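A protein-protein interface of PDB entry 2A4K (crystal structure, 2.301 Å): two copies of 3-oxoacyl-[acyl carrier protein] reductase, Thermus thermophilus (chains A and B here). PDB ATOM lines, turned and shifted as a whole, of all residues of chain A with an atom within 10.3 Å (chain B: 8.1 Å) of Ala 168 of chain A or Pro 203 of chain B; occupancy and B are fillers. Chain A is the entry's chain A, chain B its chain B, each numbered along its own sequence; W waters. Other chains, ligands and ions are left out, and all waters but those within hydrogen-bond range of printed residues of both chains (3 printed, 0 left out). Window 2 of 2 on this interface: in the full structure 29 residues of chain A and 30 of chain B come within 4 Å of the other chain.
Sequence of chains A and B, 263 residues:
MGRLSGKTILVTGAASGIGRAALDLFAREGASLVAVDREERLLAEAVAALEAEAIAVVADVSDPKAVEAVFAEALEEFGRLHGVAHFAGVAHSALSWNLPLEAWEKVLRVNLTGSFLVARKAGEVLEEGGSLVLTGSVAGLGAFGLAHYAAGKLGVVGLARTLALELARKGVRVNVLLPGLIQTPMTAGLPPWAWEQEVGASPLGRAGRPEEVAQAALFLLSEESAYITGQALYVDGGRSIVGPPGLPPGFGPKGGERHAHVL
Water W3 lies within hydrogen-bond range of OG of Ser 240 of chain B, NE2 of Gln 231 of chain A and NH1 of Arg 161 of chain A. Water W2 bridges OD1 of Asp 236 of chain B (2.7 Å) and N of Thr 229 of chain A (3.3 Å). Water W1 bridges OH of Tyr 227 of chain A and O of Asp 236 of chain B.
The side-chain hydroxyl (OH) of Tyr 227 of chain A lies within hydrogen-bond range of the backbone carbonyl oxygen (O) of Arg 206 of chain B (2.7 Å). N of Gly 237 of chain B sits at hydrogen-bond distance from O of Tyr 227 of chain A, 2.9 Å away.
Of the printed residues of chain B, Ala 168 of chain A touches Pro 203 and Leu 204. Of chain A, only Tyr 227 comes within 4 Å of Ser 202 of chain B. Gly 237 of chain B touches two residues of chain A. Of the printed residues of chain B, Thr 229 of chain A touches Gly 237 (3.6 Å), Gly 238 (3.7 Å) and Ile 241 (3.8 Å). Printed residues of chain B within 4 Å of Ala 226 of chain A: Leu 204 (3.7 Å) and Arg 206 (3.6 Å). Gly 200 of chain B touches none of the printed residues of chain A. Glu 128 of chain A touches none of the printed residues of chain B.
The backbone NH (N) of Val 174 of chain A is in hydrogen-bond range of the side-chain hydroxyl (OG1) of Thr 229 of chain A (3.0 Å). N of Leu 204 of chain B lies close to OG of Ser 202 of chain B (3.3 Å). The side-chain hydroxyl (OG) of Ser 202 of chain B is in hydrogen-bond range of the backbone carbonyl oxygen (O) of Arg 206 of chain B (2.9 Å). N of Leu 204 of chain B lies within hydrogen-bond range of O of Gly 237 of chain B. The side-chain carboxylate of Asp 236 of chain B lies within hydrogen-bond range of the backbone NH of Gly 238 of chain B, 3.0 Å away.
Of the 28 printed residues of chain A, 7 touch a printed residue of chain B. Printed residues of chain A that touch a printed residue of chain B: Arg 161, Leu 165, Ala 168, Ala 226, Tyr 227, Thr 229 and Gly 230. Hydrophobic or aromatic side chains of chain A within 4 Å of the printed part of chain B: Leu 165, Ala 168 and Tyr 227. Of the 15 printed residues of chain B, 8 touch a printed residue of chain A. Among the printed residues, 15 pairs touch across the chains. Among the printed residues, no Asp or Glu carboxylate lies within 4 Å of a Lys or Arg side-chain nitrogen of the other chain.
Leu 165 of chain A touches Pro 203 of chain B (CD2 to CG, 3.9 Å). Ile 241 of chain B touches Leu 165 of chain A. CD2 of Leu 204 of chain B touches O of Ala 168 of chain A (3.9 Å). Ala 226 of chain A touches Leu 204 of chain B. Ala 226 of chain A touches Arg 206 of chain B. OH of Tyr 227 of chain A touches OG of Ser 202 of chain B (3.5 Å). CE2 of Tyr 227 of chain A touches C of Asp 236 of chain B, 3.4 Å away. Thr 229 of chain A touches Ile 241 of chain B (O to CD1, 3.8 Å). Gly 230 of chain A touches Ile 241 of chain B (CA to CD1, 3.7 Å).
No position is printed for both chains. Of the 15 pairs that touch across the chains among the printed residues, none has its exchanged pair printed and touching as well.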
ATOM      1  N   GLY A 123      -2.410 -20.038  20.507  1.00  0.00           N
ATOM      2  CA  GLY A 123      -1.984 -21.130  19.652  1.00  0.00           C
ATOM      3  C   GLY A 123      -0.833 -21.949  20.221  1.00  0.00           C
ATOM      4  O   GLY A 123      -0.796 -23.181  20.059  1.00  0.00           O
ATOM      5  N   LEU A 126      -2.459 -23.500  24.177  1.00  0.00           N
ATOM      6  CA  LEU A 126      -3.662 -24.329  24.150  1.00  0.00           C
ATOM      7  C   LEU A 126      -3.317 -25.765  23.821  1.00  0.00           C
ATOM      8  O   LEU A 126      -2.501 -26.034  22.950  1.00  0.00           O
ATOM      9  CB  LEU A 126      -4.686 -23.804  23.146  1.00  0.00           C
ATOM     10  CG  LEU A 126      -5.518 -22.593  23.576  1.00  0.00           C
ATOM     11  CD1 LEU A 126      -6.324 -22.057  22.370  1.00  0.00           C
ATOM     12  CD2 LEU A 126      -6.431 -22.943  24.750  1.00  0.00           C
ATOM     13  N   GLU A 127      -3.928 -26.695  24.530  1.00  0.00           N
ATOM     14  CA  GLU A 127      -3.624 -28.092  24.270  1.00  0.00           C
ATOM     15  C   GLU A 127      -4.620 -28.700  23.302  1.00  0.00           C
ATOM     16  O   GLU A 127      -5.596 -28.045  22.910  1.00  0.00           O
ATOM     17  CB  GLU A 127      -3.556 -28.878  25.572  1.00  0.00           C
ATOM     18  CG  GLU A 127      -4.696 -28.647  26.550  1.00  0.00           C
ATOM     19  CD  GLU A 127      -4.612 -29.626  27.697  1.00  0.00           C
ATOM     20  OE1 GLU A 127      -3.516 -29.716  28.305  1.00  0.00           O
ATOM     21  OE2 GLU A 127      -5.621 -30.316  27.971  1.00  0.00           O
ATOM     22  N   GLU A 128      -4.357 -29.947  22.920  1.00  0.00           N
ATOM     23  CA  GLU A 128      -5.217 -30.708  22.013  1.00  0.00           C
ATOM     24  C   GLU A 128      -6.684 -30.584  22.408  1.00  0.00           C
ATOM     25  O   GLU A 128      -7.020 -30.751  23.574  1.00  0.00           O
ATOM     26  CB  GLU A 128      -4.794 -32.185  21.983  1.00  0.00           C
ATOM     27  CG  GLU A 128      -3.286 -32.404  21.714  1.00  0.00           C
ATOM     28  N   GLY A 129      -7.536 -30.280  21.427  1.00  0.00           N
ATOM     29  CA  GLY A 129      -8.979 -30.101  21.639  1.00  0.00           C
ATOM     30  C   GLY A 129      -9.378 -28.714  22.140  1.00  0.00           C
ATOM     31  O   GLY A 129     -10.572 -28.456  22.376  1.00  0.00           O
ATOM     32  N   GLY A 130      -8.393 -27.824  22.305  1.00  0.00           N
ATOM     33  CA  GLY A 130      -8.644 -26.451  22.783  1.00  0.00           C
ATOM     34  C   GLY A 130      -9.385 -25.566  21.791  1.00  0.00           C
ATOM     35  O   GLY A 130      -9.559 -25.928  20.607  1.00  0.00           O
ATOM     36  N   LEU A 132      -9.935 -21.399  20.616  1.00  0.00           N
ATOM     37  CA  LEU A 132      -9.709 -19.961  20.589  1.00  0.00           C
ATOM     38  C   LEU A 132     -10.862 -19.233  19.863  1.00  0.00           C
ATOM     39  O   LEU A 132     -11.142 -19.515  18.693  1.00  0.00           O
ATOM     40  CB  LEU A 132      -8.375 -19.651  19.913  1.00  0.00           C
ATOM     41  CG  LEU A 132      -8.022 -18.204  19.516  1.00  0.00           C
ATOM     42  CD1 LEU A 132      -7.749 -17.271  20.697  1.00  0.00           C
ATOM     43  CD2 LEU A 132      -6.818 -18.250  18.609  1.00  0.00           C
ATOM     44  N   ALA A 160      -8.163 -15.779  11.675  1.00  0.00           N
ATOM     45  CA  ALA A 160      -8.804 -16.993  12.217  1.00  0.00           C
ATOM     46  C   ALA A 160      -8.786 -18.189  11.260  1.00  0.00           C
ATOM     47  O   ALA A 160      -8.511 -19.317  11.676  1.00  0.00           O
ATOM     48  CB  ALA A 160     -10.256 -16.686  12.649  1.00  0.00           C
ATOM     49  N   ARG A 161      -9.075 -17.938   9.986  1.00  0.00           N
ATOM     50  CA  ARG A 161      -9.091 -19.002   8.988  1.00  0.00           C
ATOM     51  C   ARG A 161      -7.686 -19.543   8.703  1.00  0.00           C
ATOM     52  O   ARG A 161      -7.515 -20.756   8.569  1.00  0.00           O
ATOM     53  CB  ARG A 161      -9.866 -18.583   7.724  1.00  0.00           C
ATOM     54  CG  ARG A 161     -11.372 -18.811   7.890  1.00  0.00           C
ATOM     55  CD  ARG A 161     -12.247 -18.153   6.825  1.00  0.00           C
ATOM     56  NE  ARG A 161     -12.196 -18.772   5.498  1.00  0.00           N
ATOM     57  CZ  ARG A 161     -12.969 -19.778   5.069  1.00  0.00           C
ATOM     58  NH1 ARG A 161     -13.883 -20.350   5.859  1.00  0.00           N
ATOM     59  NH2 ARG A 161     -12.813 -20.222   3.826  1.00  0.00           N
ATOM     60  N   THR A 162      -6.694 -18.645   8.649  1.00  0.00           N
ATOM     61  CA  THR A 162      -5.269 -19.012   8.520  1.00  0.00           C
ATOM     62  C   THR A 162      -4.789 -19.784   9.745  1.00  0.00           C
ATOM     63  O   THR A 162      -4.150 -20.809   9.600  1.00  0.00           O
ATOM     64  CB  THR A 162      -4.370 -17.749   8.297  1.00  0.00           C
ATOM     65  OG1 THR A 162      -4.743 -17.128   7.068  1.00  0.00           O
ATOM     66  CG2 THR A 162      -2.885 -18.097   8.231  1.00  0.00           C
ATOM     67  N   LEU A 163      -5.096 -19.297  10.944  1.00  0.00           N
ATOM     68  CA  LEU A 163      -4.710 -20.013  12.172  1.00  0.00           C
ATOM     69  C   LEU A 163      -5.415 -21.374  12.326  1.00  0.00           C
ATOM     70  O   LEU A 163      -4.792 -22.335  12.751  1.00  0.00           O
ATOM     71  CB  LEU A 163      -4.936 -19.161  13.425  1.00  0.00           C
ATOM     72  CG  LEU A 163      -3.860 -18.224  13.970  1.00  0.00           C
ATOM     73  CD1 LEU A 163      -4.271 -17.879  15.354  1.00  0.00           C
ATOM     74  CD2 LEU A 163      -2.453 -18.861  14.026  1.00  0.00           C
ATOM     75  N   ALA A 164      -6.702 -21.440  11.972  1.00  0.00           N
ATOM     76  CA  ALA A 164      -7.466 -22.703  12.002  1.00  0.00           C
ATOM     77  C   ALA A 164      -6.733 -23.819  11.246  1.00  0.00           C
ATOM     78  O   ALA A 164      -6.603 -24.924  11.767  1.00  0.00           O
ATOM     79  CB  ALA A 164      -8.879 -22.510  11.437  1.00  0.00           C
ATOM     80  N   LEU A 165      -6.247 -23.506  10.039  1.00  0.00           N
ATOM     81  CA  LEU A 165      -5.457 -24.451   9.234  1.00  0.00           C
ATOM     82  C   LEU A 165      -4.121 -24.860   9.882  1.00  0.00           C
ATOM     83  O   LEU A 165      -3.741 -26.035   9.856  1.00  0.00           O
ATOM     84  CB  LEU A 165      -5.228 -23.914   7.815  1.00  0.00           C
ATOM     85  CG  LEU A 165      -6.434 -23.745   6.895  1.00  0.00           C
ATOM     86  CD1 LEU A 165      -5.971 -23.343   5.484  1.00  0.00           C
ATOM     87  CD2 LEU A 165      -7.308 -25.019   6.841  1.00  0.00           C
ATOM     88  N   GLU A 166      -3.431 -23.894  10.469  1.00  0.00           N
ATOM     89  CA  GLU A 166      -2.125 -24.135  11.081  1.00  0.00           C
ATOM     90  C   GLU A 166      -2.203 -24.944  12.383  1.00  0.00           C
ATOM     91  O   GLU A 166      -1.352 -25.804  12.605  1.00  0.00           O
ATOM     92  CB  GLU A 166      -1.390 -22.803  11.299  1.00  0.00           C
ATOM     93  CG  GLU A 166      -1.132 -22.039   9.976  1.00  0.00           C
ATOM     94  CD  GLU A 166      -0.408 -20.692  10.151  1.00  0.00           C
ATOM     95  OE1 GLU A 166      -0.468 -20.089  11.254  1.00  0.00           O
ATOM     96  OE2 GLU A 166       0.212 -20.237   9.156  1.00  0.00           O
ATOM     97  N   LEU A 167      -3.224 -24.669  13.214  1.00  0.00           N
ATOM     98  CA  LEU A 167      -3.420 -25.294  14.548  1.00  0.00           C
ATOM     99  C   LEU A 167      -4.238 -26.595  14.560  1.00  0.00           C
ATOM    100  O   LEU A 167      -4.278 -27.306  15.568  1.00  0.00           O
ATOM    101  CB  LEU A 167      -4.064 -24.276  15.511  1.00  0.00           C
ATOM    102  CG  LEU A 167      -3.299 -22.976  15.796  1.00  0.00           C
ATOM    103  CD1 LEU A 167      -4.105 -22.083  16.689  1.00  0.00           C
ATOM    104  CD2 LEU A 167      -1.897 -23.246  16.415  1.00  0.00           C
ATOM    105  N   ALA A 168      -4.895 -26.897  13.445  1.00  0.00           N
ATOM    106  CA  ALA A 168      -5.702 -28.105  13.291  1.00  0.00           C
ATOM    107  C   ALA A 168      -4.893 -29.403  13.561  1.00  0.00           C
ATOM    108  O   ALA A 168      -5.449 -30.405  14.015  1.00  0.00           O
ATOM    109  CB  ALA A 168      -6.314 -28.137  11.894  1.00  0.00           C
ATOM    110  N   ARG A 169      -3.589 -29.373  13.295  1.00  0.00           N
ATOM    111  CA  ARG A 169      -2.727 -30.542  13.551  1.00  0.00           C
ATOM    112  C   ARG A 169      -2.600 -30.814  15.052  1.00  0.00           C
ATOM    113  O   ARG A 169      -2.673 -31.957  15.487  1.00  0.00           O
ATOM    114  CB  ARG A 169      -1.347 -30.363  12.913  1.00  0.00           C
ATOM    115  N   LYS A 170      -2.430 -29.745  15.825  1.00  0.00           N
ATOM    116  CA  LYS A 170      -2.419 -29.780  17.290  1.00  0.00           C
ATOM    117  C   LYS A 170      -3.828 -30.061  17.876  1.00  0.00           C
ATOM    118  O   LYS A 170      -3.972 -30.254  19.077  1.00  0.00           O
ATOM    119  CB  LYS A 170      -1.857 -28.431  17.782  1.00  0.00           C
ATOM    120  CG  LYS A 170      -1.472 -28.283  19.267  1.00  0.00           C
ATOM    121  CD  LYS A 170      -0.795 -26.914  19.456  1.00  0.00           C
ATOM    122  CE  LYS A 170      -0.598 -26.507  20.916  1.00  0.00           C
ATOM    123  NZ  LYS A 170       0.350 -27.366  21.725  1.00  0.00           N
ATOM    124  N   GLY A 171      -4.859 -30.082  17.026  1.00  0.00           N
ATOM    125  CA  GLY A 171      -6.249 -30.277  17.465  1.00  0.00           C
ATOM    126  C   GLY A 171      -6.976 -29.017  17.968  1.00  0.00           C
ATOM    127  O   GLY A 171      -8.091 -29.117  18.508  1.00  0.00           O
ATOM    128  N   VAL A 172      -6.364 -27.841  17.785  1.00  0.00           N
ATOM    129  CA  VAL A 172      -6.936 -26.583  18.284  1.00  0.00           C
ATOM    130  C   VAL A 172      -7.901 -25.964  17.256  1.00  0.00           C
ATOM    131  O   VAL A 172      -7.558 -25.778  16.083  1.00  0.00           O
ATOM    132  CB  VAL A 172      -5.831 -25.548  18.734  1.00  0.00           C
ATOM    133  CG1 VAL A 172      -6.442 -24.294  19.319  1.00  0.00           C
ATOM    134  CG2 VAL A 172      -4.889 -26.164  19.763  1.00  0.00           C
ATOM    135  N   ARG A 173      -9.107 -25.642  17.724  1.00  0.00           N
ATOM    136  CA  ARG A 173     -10.119 -24.946  16.914  1.00  0.00           C
ATOM    137  C   ARG A 173     -10.007 -23.416  16.995  1.00  0.00           C
ATOM    138  O   ARG A 173      -9.662 -22.849  18.052  1.00  0.00           O
ATOM    139  CB  ARG A 173     -11.495 -25.405  17.365  1.00  0.00           C
ATOM    140  CG  ARG A 173     -11.527 -26.925  17.536  1.00  0.00           C
ATOM    141  CD  ARG A 173     -12.857 -27.447  17.877  1.00  0.00           C
ATOM    142  NE  ARG A 173     -13.279 -27.250  19.268  1.00  0.00           N
ATOM    143  CZ  ARG A 173     -14.211 -26.381  19.652  1.00  0.00           C
ATOM    144  NH1 ARG A 173     -14.797 -25.565  18.737  1.00  0.00           N
ATOM    145  NH2 ARG A 173     -14.563 -26.319  20.943  1.00  0.00           N
ATOM    146  N   VAL A 174     -10.269 -22.744  15.873  1.00  0.00           N
ATOM    147  CA  VAL A 174     -10.273 -21.287  15.835  1.00  0.00           C
ATOM    148  C   VAL A 174     -11.493 -20.835  15.059  1.00  0.00           C
ATOM    149  O   VAL A 174     -11.711 -21.253  13.927  1.00  0.00           O
ATOM    150  CB  VAL A 174      -8.965 -20.647  15.266  1.00  0.00           C
ATOM    151  CG1 VAL A 174      -8.973 -19.113  15.470  1.00  0.00           C
ATOM    152  CG2 VAL A 174      -7.714 -21.249  15.924  1.00  0.00           C
ATOM    153  N   ALA A 226     -16.963 -29.425  18.963  1.00  0.00           N
ATOM    154  CA  ALA A 226     -15.618 -30.027  18.756  1.00  0.00           C
ATOM    155  C   ALA A 226     -15.229 -30.244  17.288  1.00  0.00           C
ATOM    156  O   ALA A 226     -14.062 -30.390  16.988  1.00  0.00           O
ATOM    157  CB  ALA A 226     -15.485 -31.366  19.546  1.00  0.00           C
ATOM    158  N   TYR A 227     -16.188 -30.266  16.371  1.00  0.00           N
ATOM    159  CA  TYR A 227     -15.833 -30.488  14.951  1.00  0.00           C
ATOM    160  C   TYR A 227     -15.942 -29.207  14.100  1.00  0.00           C
ATOM    161  O   TYR A 227     -16.006 -29.271  12.872  1.00  0.00           O
ATOM    162  CB  TYR A 227     -16.665 -31.646  14.353  1.00  0.00           C
ATOM    163  CG  TYR A 227     -16.090 -32.297  13.090  1.00  0.00           C
ATOM    164  CD1 TYR A 227     -14.776 -32.789  13.049  1.00  0.00           C
ATOM    165  CD2 TYR A 227     -16.874 -32.448  11.956  1.00  0.00           C
ATOM    166  CE1 TYR A 227     -14.256 -33.407  11.882  1.00  0.00           C
ATOM    167  CE2 TYR A 227     -16.376 -33.061  10.790  1.00  0.00           C
ATOM    168  CZ  TYR A 227     -15.077 -33.535  10.766  1.00  0.00           C
ATOM    169  OH  TYR A 227     -14.609 -34.128   9.609  1.00  0.00           O
ATOM    170  N   ILE A 228     -15.976 -28.052  14.770  1.00  0.00           N
ATOM    171  CA  ILE A 228     -16.198 -26.768  14.100  1.00  0.00           C
ATOM    172  C   ILE A 228     -14.963 -25.848  14.226  1.00  0.00           C
ATOM    173  O   ILE A 228     -14.559 -25.458  15.349  1.00  0.00           O
ATOM    174  CB  ILE A 228     -17.493 -26.028  14.634  1.00  0.00           C
ATOM    175  CG1 ILE A 228     -18.735 -26.962  14.649  1.00  0.00           C
ATOM    176  CG2 ILE A 228     -17.730 -24.769  13.832  1.00  0.00           C
ATOM    177  CD1 ILE A 228     -20.061 -26.319  15.084  1.00  0.00           C
ATOM    178  N   THR A 229     -14.388 -25.496  13.068  1.00  0.00           N
ATOM    179  CA  THR A 229     -13.252 -24.590  13.016  1.00  0.00           C
ATOM    180  C   THR A 229     -13.238 -23.797  11.696  1.00  0.00           C
ATOM    181  O   THR A 229     -13.783 -24.257  10.691  1.00  0.00           O
ATOM    182  CB  THR A 229     -11.897 -25.325  13.265  1.00  0.00           C
ATOM    183  OG1 THR A 229     -10.874 -24.348  13.389  1.00  0.00           O
ATOM    184  CG2 THR A 229     -11.517 -26.278  12.094  1.00  0.00           C
ATOM    185  N   GLY A 230     -12.622 -22.610  11.726  1.00  0.00           N
ATOM    186  CA  GLY A 230     -12.613 -21.673  10.601  1.00  0.00           C
ATOM    187  C   GLY A 230     -13.907 -20.897  10.327  1.00  0.00           C
ATOM    188  O   GLY A 230     -14.055 -20.290   9.251  1.00  0.00           O
ATOM    189  N   GLN A 231     -14.841 -20.903  11.282  1.00  0.00           N
ATOM    190  CA  GLN A 231     -16.167 -20.313  11.058  1.00  0.00           C
ATOM    191  C   GLN A 231     -16.340 -18.881  11.582  1.00  0.00           C
ATOM    192  O   GLN A 231     -15.851 -18.543  12.655  1.00  0.00           O
ATOM    193  CB  GLN A 231     -17.256 -21.220  11.686  1.00  0.00           C
ATOM    194  CG  GLN A 231     -17.299 -22.637  11.088  1.00  0.00           C
ATOM    195  CD  GLN A 231     -17.488 -22.598   9.592  1.00  0.00           C
ATOM    196  OE1 GLN A 231     -18.532 -22.153   9.099  1.00  0.00           O
ATOM    197  NE2 GLN A 231     -16.465 -23.045   8.851  1.00  0.00           N
ATOM    198  N   GLU B 198      -9.610 -41.827   7.116  1.00  0.00           N
ATOM    199  CA  GLU B 198     -10.438 -40.750   7.696  1.00  0.00           C
ATOM    200  C   GLU B 198      -9.625 -39.521   8.143  1.00  0.00           C
ATOM    201  O   GLU B 198     -10.176 -38.438   8.241  1.00  0.00           O
ATOM    202  CB  GLU B 198     -11.331 -41.273   8.831  1.00  0.00           C
ATOM    203  CG  GLU B 198     -12.335 -42.335   8.352  1.00  0.00           C
ATOM    204  CD  GLU B 198     -13.550 -42.480   9.242  1.00  0.00           C
ATOM    205  OE1 GLU B 198     -13.441 -42.316  10.476  1.00  0.00           O
ATOM    206  OE2 GLU B 198     -14.628 -42.772   8.695  1.00  0.00           O
ATOM    207  N   VAL B 199      -8.327 -39.708   8.392  1.00  0.00           N
ATOM    208  CA  VAL B 199      -7.386 -38.623   8.710  1.00  0.00           C
ATOM    209  C   VAL B 199      -7.407 -37.500   7.647  1.00  0.00           C
ATOM    210  O   VAL B 199      -7.305 -36.311   7.992  1.00  0.00           O
ATOM    211  CB  VAL B 199      -5.916 -39.154   8.932  1.00  0.00           C
ATOM    212  CG1 VAL B 199      -4.947 -38.024   9.281  1.00  0.00           C
ATOM    213  CG2 VAL B 199      -5.870 -40.215  10.033  1.00  0.00           C
ATOM    214  N   GLY B 200      -7.562 -37.876   6.376  1.00  0.00           N
ATOM    215  CA  GLY B 200      -7.578 -36.913   5.269  1.00  0.00           C
ATOM    216  C   GLY B 200      -8.928 -36.266   4.980  1.00  0.00           C
ATOM    217  O   GLY B 200      -9.069 -35.549   3.971  1.00  0.00           O
ATOM    218  N   ALA B 201      -9.920 -36.520   5.844  1.00  0.00           N
ATOM    219  CA  ALA B 201     -11.278 -35.982   5.668  1.00  0.00           C
ATOM    220  C   ALA B 201     -11.364 -34.477   5.963  1.00  0.00           C
ATOM    221  O   ALA B 201     -12.187 -33.780   5.370  1.00  0.00           O
ATOM    222  CB  ALA B 201     -12.298 -36.753   6.515  1.00  0.00           C
ATOM    223  N   SER B 202     -10.512 -33.990   6.866  1.00  0.00           N
ATOM    224  CA  SER B 202     -10.535 -32.590   7.292  1.00  0.00           C
ATOM    225  C   SER B 202      -9.222 -32.201   7.935  1.00  0.00           C
ATOM    226  O   SER B 202      -8.488 -33.088   8.409  1.00  0.00           O
ATOM    227  CB  SER B 202     -11.669 -32.363   8.312  1.00  0.00           C
ATOM    228  OG  SER B 202     -11.298 -32.894   9.572  1.00  0.00           O
ATOM    229  N   PRO B 203      -8.910 -30.879   7.971  1.00  0.00           N
ATOM    230  CA  PRO B 203      -7.726 -30.415   8.725  1.00  0.00           C
ATOM    231  C   PRO B 203      -7.616 -30.991  10.145  1.00  0.00           C
ATOM    232  O   PRO B 203      -6.512 -31.276  10.591  1.00  0.00           O
ATOM    233  CB  PRO B 203      -7.895 -28.888   8.754  1.00  0.00           C
ATOM    234  CG  PRO B 203      -8.749 -28.571   7.538  1.00  0.00           C
ATOM    235  CD  PRO B 203      -9.599 -29.769   7.269  1.00  0.00           C
ATOM    236  N   LEU B 204      -8.735 -31.172  10.852  1.00  0.00           N
ATOM    237  CA  LEU B 204      -8.697 -31.755  12.203  1.00  0.00           C
ATOM    238  C   LEU B 204      -8.320 -33.247  12.229  1.00  0.00           C
ATOM    239  O   LEU B 204      -8.217 -33.831  13.292  1.00  0.00           O
ATOM    240  CB  LEU B 204     -10.011 -31.502  12.974  1.00  0.00           C
ATOM    241  CG  LEU B 204     -10.301 -30.073  13.498  1.00  0.00           C
ATOM    242  CD1 LEU B 204     -11.637 -30.046  14.205  1.00  0.00           C
ATOM    243  CD2 LEU B 204      -9.221 -29.586  14.444  1.00  0.00           C
ATOM    244  N   GLY B 205      -8.125 -33.856  11.059  1.00  0.00           N
ATOM    245  CA  GLY B 205      -7.626 -35.230  10.976  1.00  0.00           C
ATOM    246  C   GLY B 205      -8.617 -36.305  11.399  1.00  0.00           C
ATOM    247  O   GLY B 205      -8.222 -37.311  12.000  1.00  0.00           O
ATOM    248  N   ARG B 206      -9.898 -36.085  11.096  1.00  0.00           N
ATOM    249  CA  ARG B 206     -10.966 -37.066  11.375  1.00  0.00           C
ATOM    250  C   ARG B 206     -12.250 -36.694  10.648  1.00  0.00           C
ATOM    251  O   ARG B 206     -12.403 -35.560  10.168  1.00  0.00           O
ATOM    252  CB  ARG B 206     -11.233 -37.215  12.884  1.00  0.00           C
ATOM    253  CG  ARG B 206     -11.907 -36.000  13.595  1.00  0.00           C
ATOM    254  CD  ARG B 206     -12.309 -36.416  15.008  1.00  0.00           C
ATOM    255  NE  ARG B 206     -12.853 -35.317  15.808  1.00  0.00           N
ATOM    256  CZ  ARG B 206     -14.149 -35.016  15.930  1.00  0.00           C
ATOM    257  NH1 ARG B 206     -15.089 -35.704  15.284  1.00  0.00           N
ATOM    258  NH2 ARG B 206     -14.503 -33.996  16.690  1.00  0.00           N
ATOM    259  N   ASP B 236     -17.645 -29.438   9.700  1.00  0.00           N
ATOM    260  CA  ASP B 236     -16.830 -30.183   8.730  1.00  0.00           C
ATOM    261  C   ASP B 236     -15.329 -30.273   9.066  1.00  0.00           C
ATOM    262  O   ASP B 236     -14.533 -30.628   8.203  1.00  0.00           O
ATOM    263  CB  ASP B 236     -17.010 -29.581   7.322  1.00  0.00           C
ATOM    264  CG  ASP B 236     -16.430 -28.166   7.190  1.00  0.00           C
ATOM    265  OD1 ASP B 236     -15.912 -27.569   8.184  1.00  0.00           O
ATOM    266  OD2 ASP B 236     -16.479 -27.643   6.062  1.00  0.00           O
ATOM    267  N   GLY B 237     -14.954 -29.943  10.301  1.00  0.00           N
ATOM    268  CA  GLY B 237     -13.554 -30.022  10.734  1.00  0.00           C
ATOM    269  C   GLY B 237     -12.597 -29.101   9.981  1.00  0.00           C
ATOM    270  O   GLY B 237     -11.396 -29.288  10.059  1.00  0.00           O
ATOM    271  N   GLY B 238     -13.137 -28.106   9.270  1.00  0.00           N
ATOM    272  CA  GLY B 238     -12.349 -27.188   8.456  1.00  0.00           C
ATOM    273  C   GLY B 238     -12.241 -27.547   6.977  1.00  0.00           C
ATOM    274  O   GLY B 238     -11.528 -26.866   6.209  1.00  0.00           O
ATOM    275  N   ARG B 239     -12.935 -28.611   6.570  1.00  0.00           N
ATOM    276  CA  ARG B 239     -12.844 -29.146   5.188  1.00  0.00           C
ATOM    277  C   ARG B 239     -13.051 -28.100   4.070  1.00  0.00           C
ATOM    278  O   ARG B 239     -12.344 -28.118   3.050  1.00  0.00           O
ATOM    279  CB  ARG B 239     -13.827 -30.314   5.027  1.00  0.00           C
ATOM    280  CG  ARG B 239     -13.851 -31.016   3.672  1.00  0.00           C
ATOM    281  CD  ARG B 239     -14.648 -32.295   3.839  1.00  0.00           C
ATOM    282  NE  ARG B 239     -14.773 -33.120   2.637  1.00  0.00           N
ATOM    283  CZ  ARG B 239     -13.911 -34.063   2.242  1.00  0.00           C
ATOM    284  NH1 ARG B 239     -12.802 -34.327   2.918  1.00  0.00           N
ATOM    285  NH2 ARG B 239     -14.162 -34.744   1.139  1.00  0.00           N
ATOM    286  N   SER B 240     -14.014 -27.201   4.287  1.00  0.00           N
ATOM    287  CA  SER B 240     -14.418 -26.159   3.324  1.00  0.00           C
ATOM    288  C   SER B 240     -13.578 -24.873   3.337  1.00  0.00           C
ATOM    289  O   SER B 240     -13.831 -23.955   2.536  1.00  0.00           O
ATOM    290  CB  SER B 240     -15.870 -25.784   3.581  1.00  0.00           C
ATOM    291  OG  SER B 240     -16.008 -25.348   4.927  1.00  0.00           O
ATOM    292  N   ILE B 241     -12.591 -24.795   4.233  1.00  0.00           N
ATOM    293  CA  ILE B 241     -11.689 -23.636   4.301  1.00  0.00           C
ATOM    294  C   ILE B 241     -10.770 -23.695   3.063  1.00  0.00           C
ATOM    295  O   ILE B 241      -9.671 -24.272   3.101  1.00  0.00           O
ATOM    296  CB  ILE B 241     -10.874 -23.600   5.624  1.00  0.00           C
ATOM    297  CG1 ILE B 241     -11.791 -23.628   6.849  1.00  0.00           C
ATOM    298  CG2 ILE B 241      -9.959 -22.372   5.692  1.00  0.00           C
ATOM    299  CD1 ILE B 241     -11.024 -23.948   8.164  1.00  0.00           C
HETATM  300  O   HOH W   1     -15.434 -33.206   7.136  1.00  0.00           O
HETATM  301  O   HOH W   2     -16.365 -26.506  10.667  1.00  0.00           O
HETATM  302  O   HOH W   3     -15.826 -22.815   5.938  1.00  0.00           O
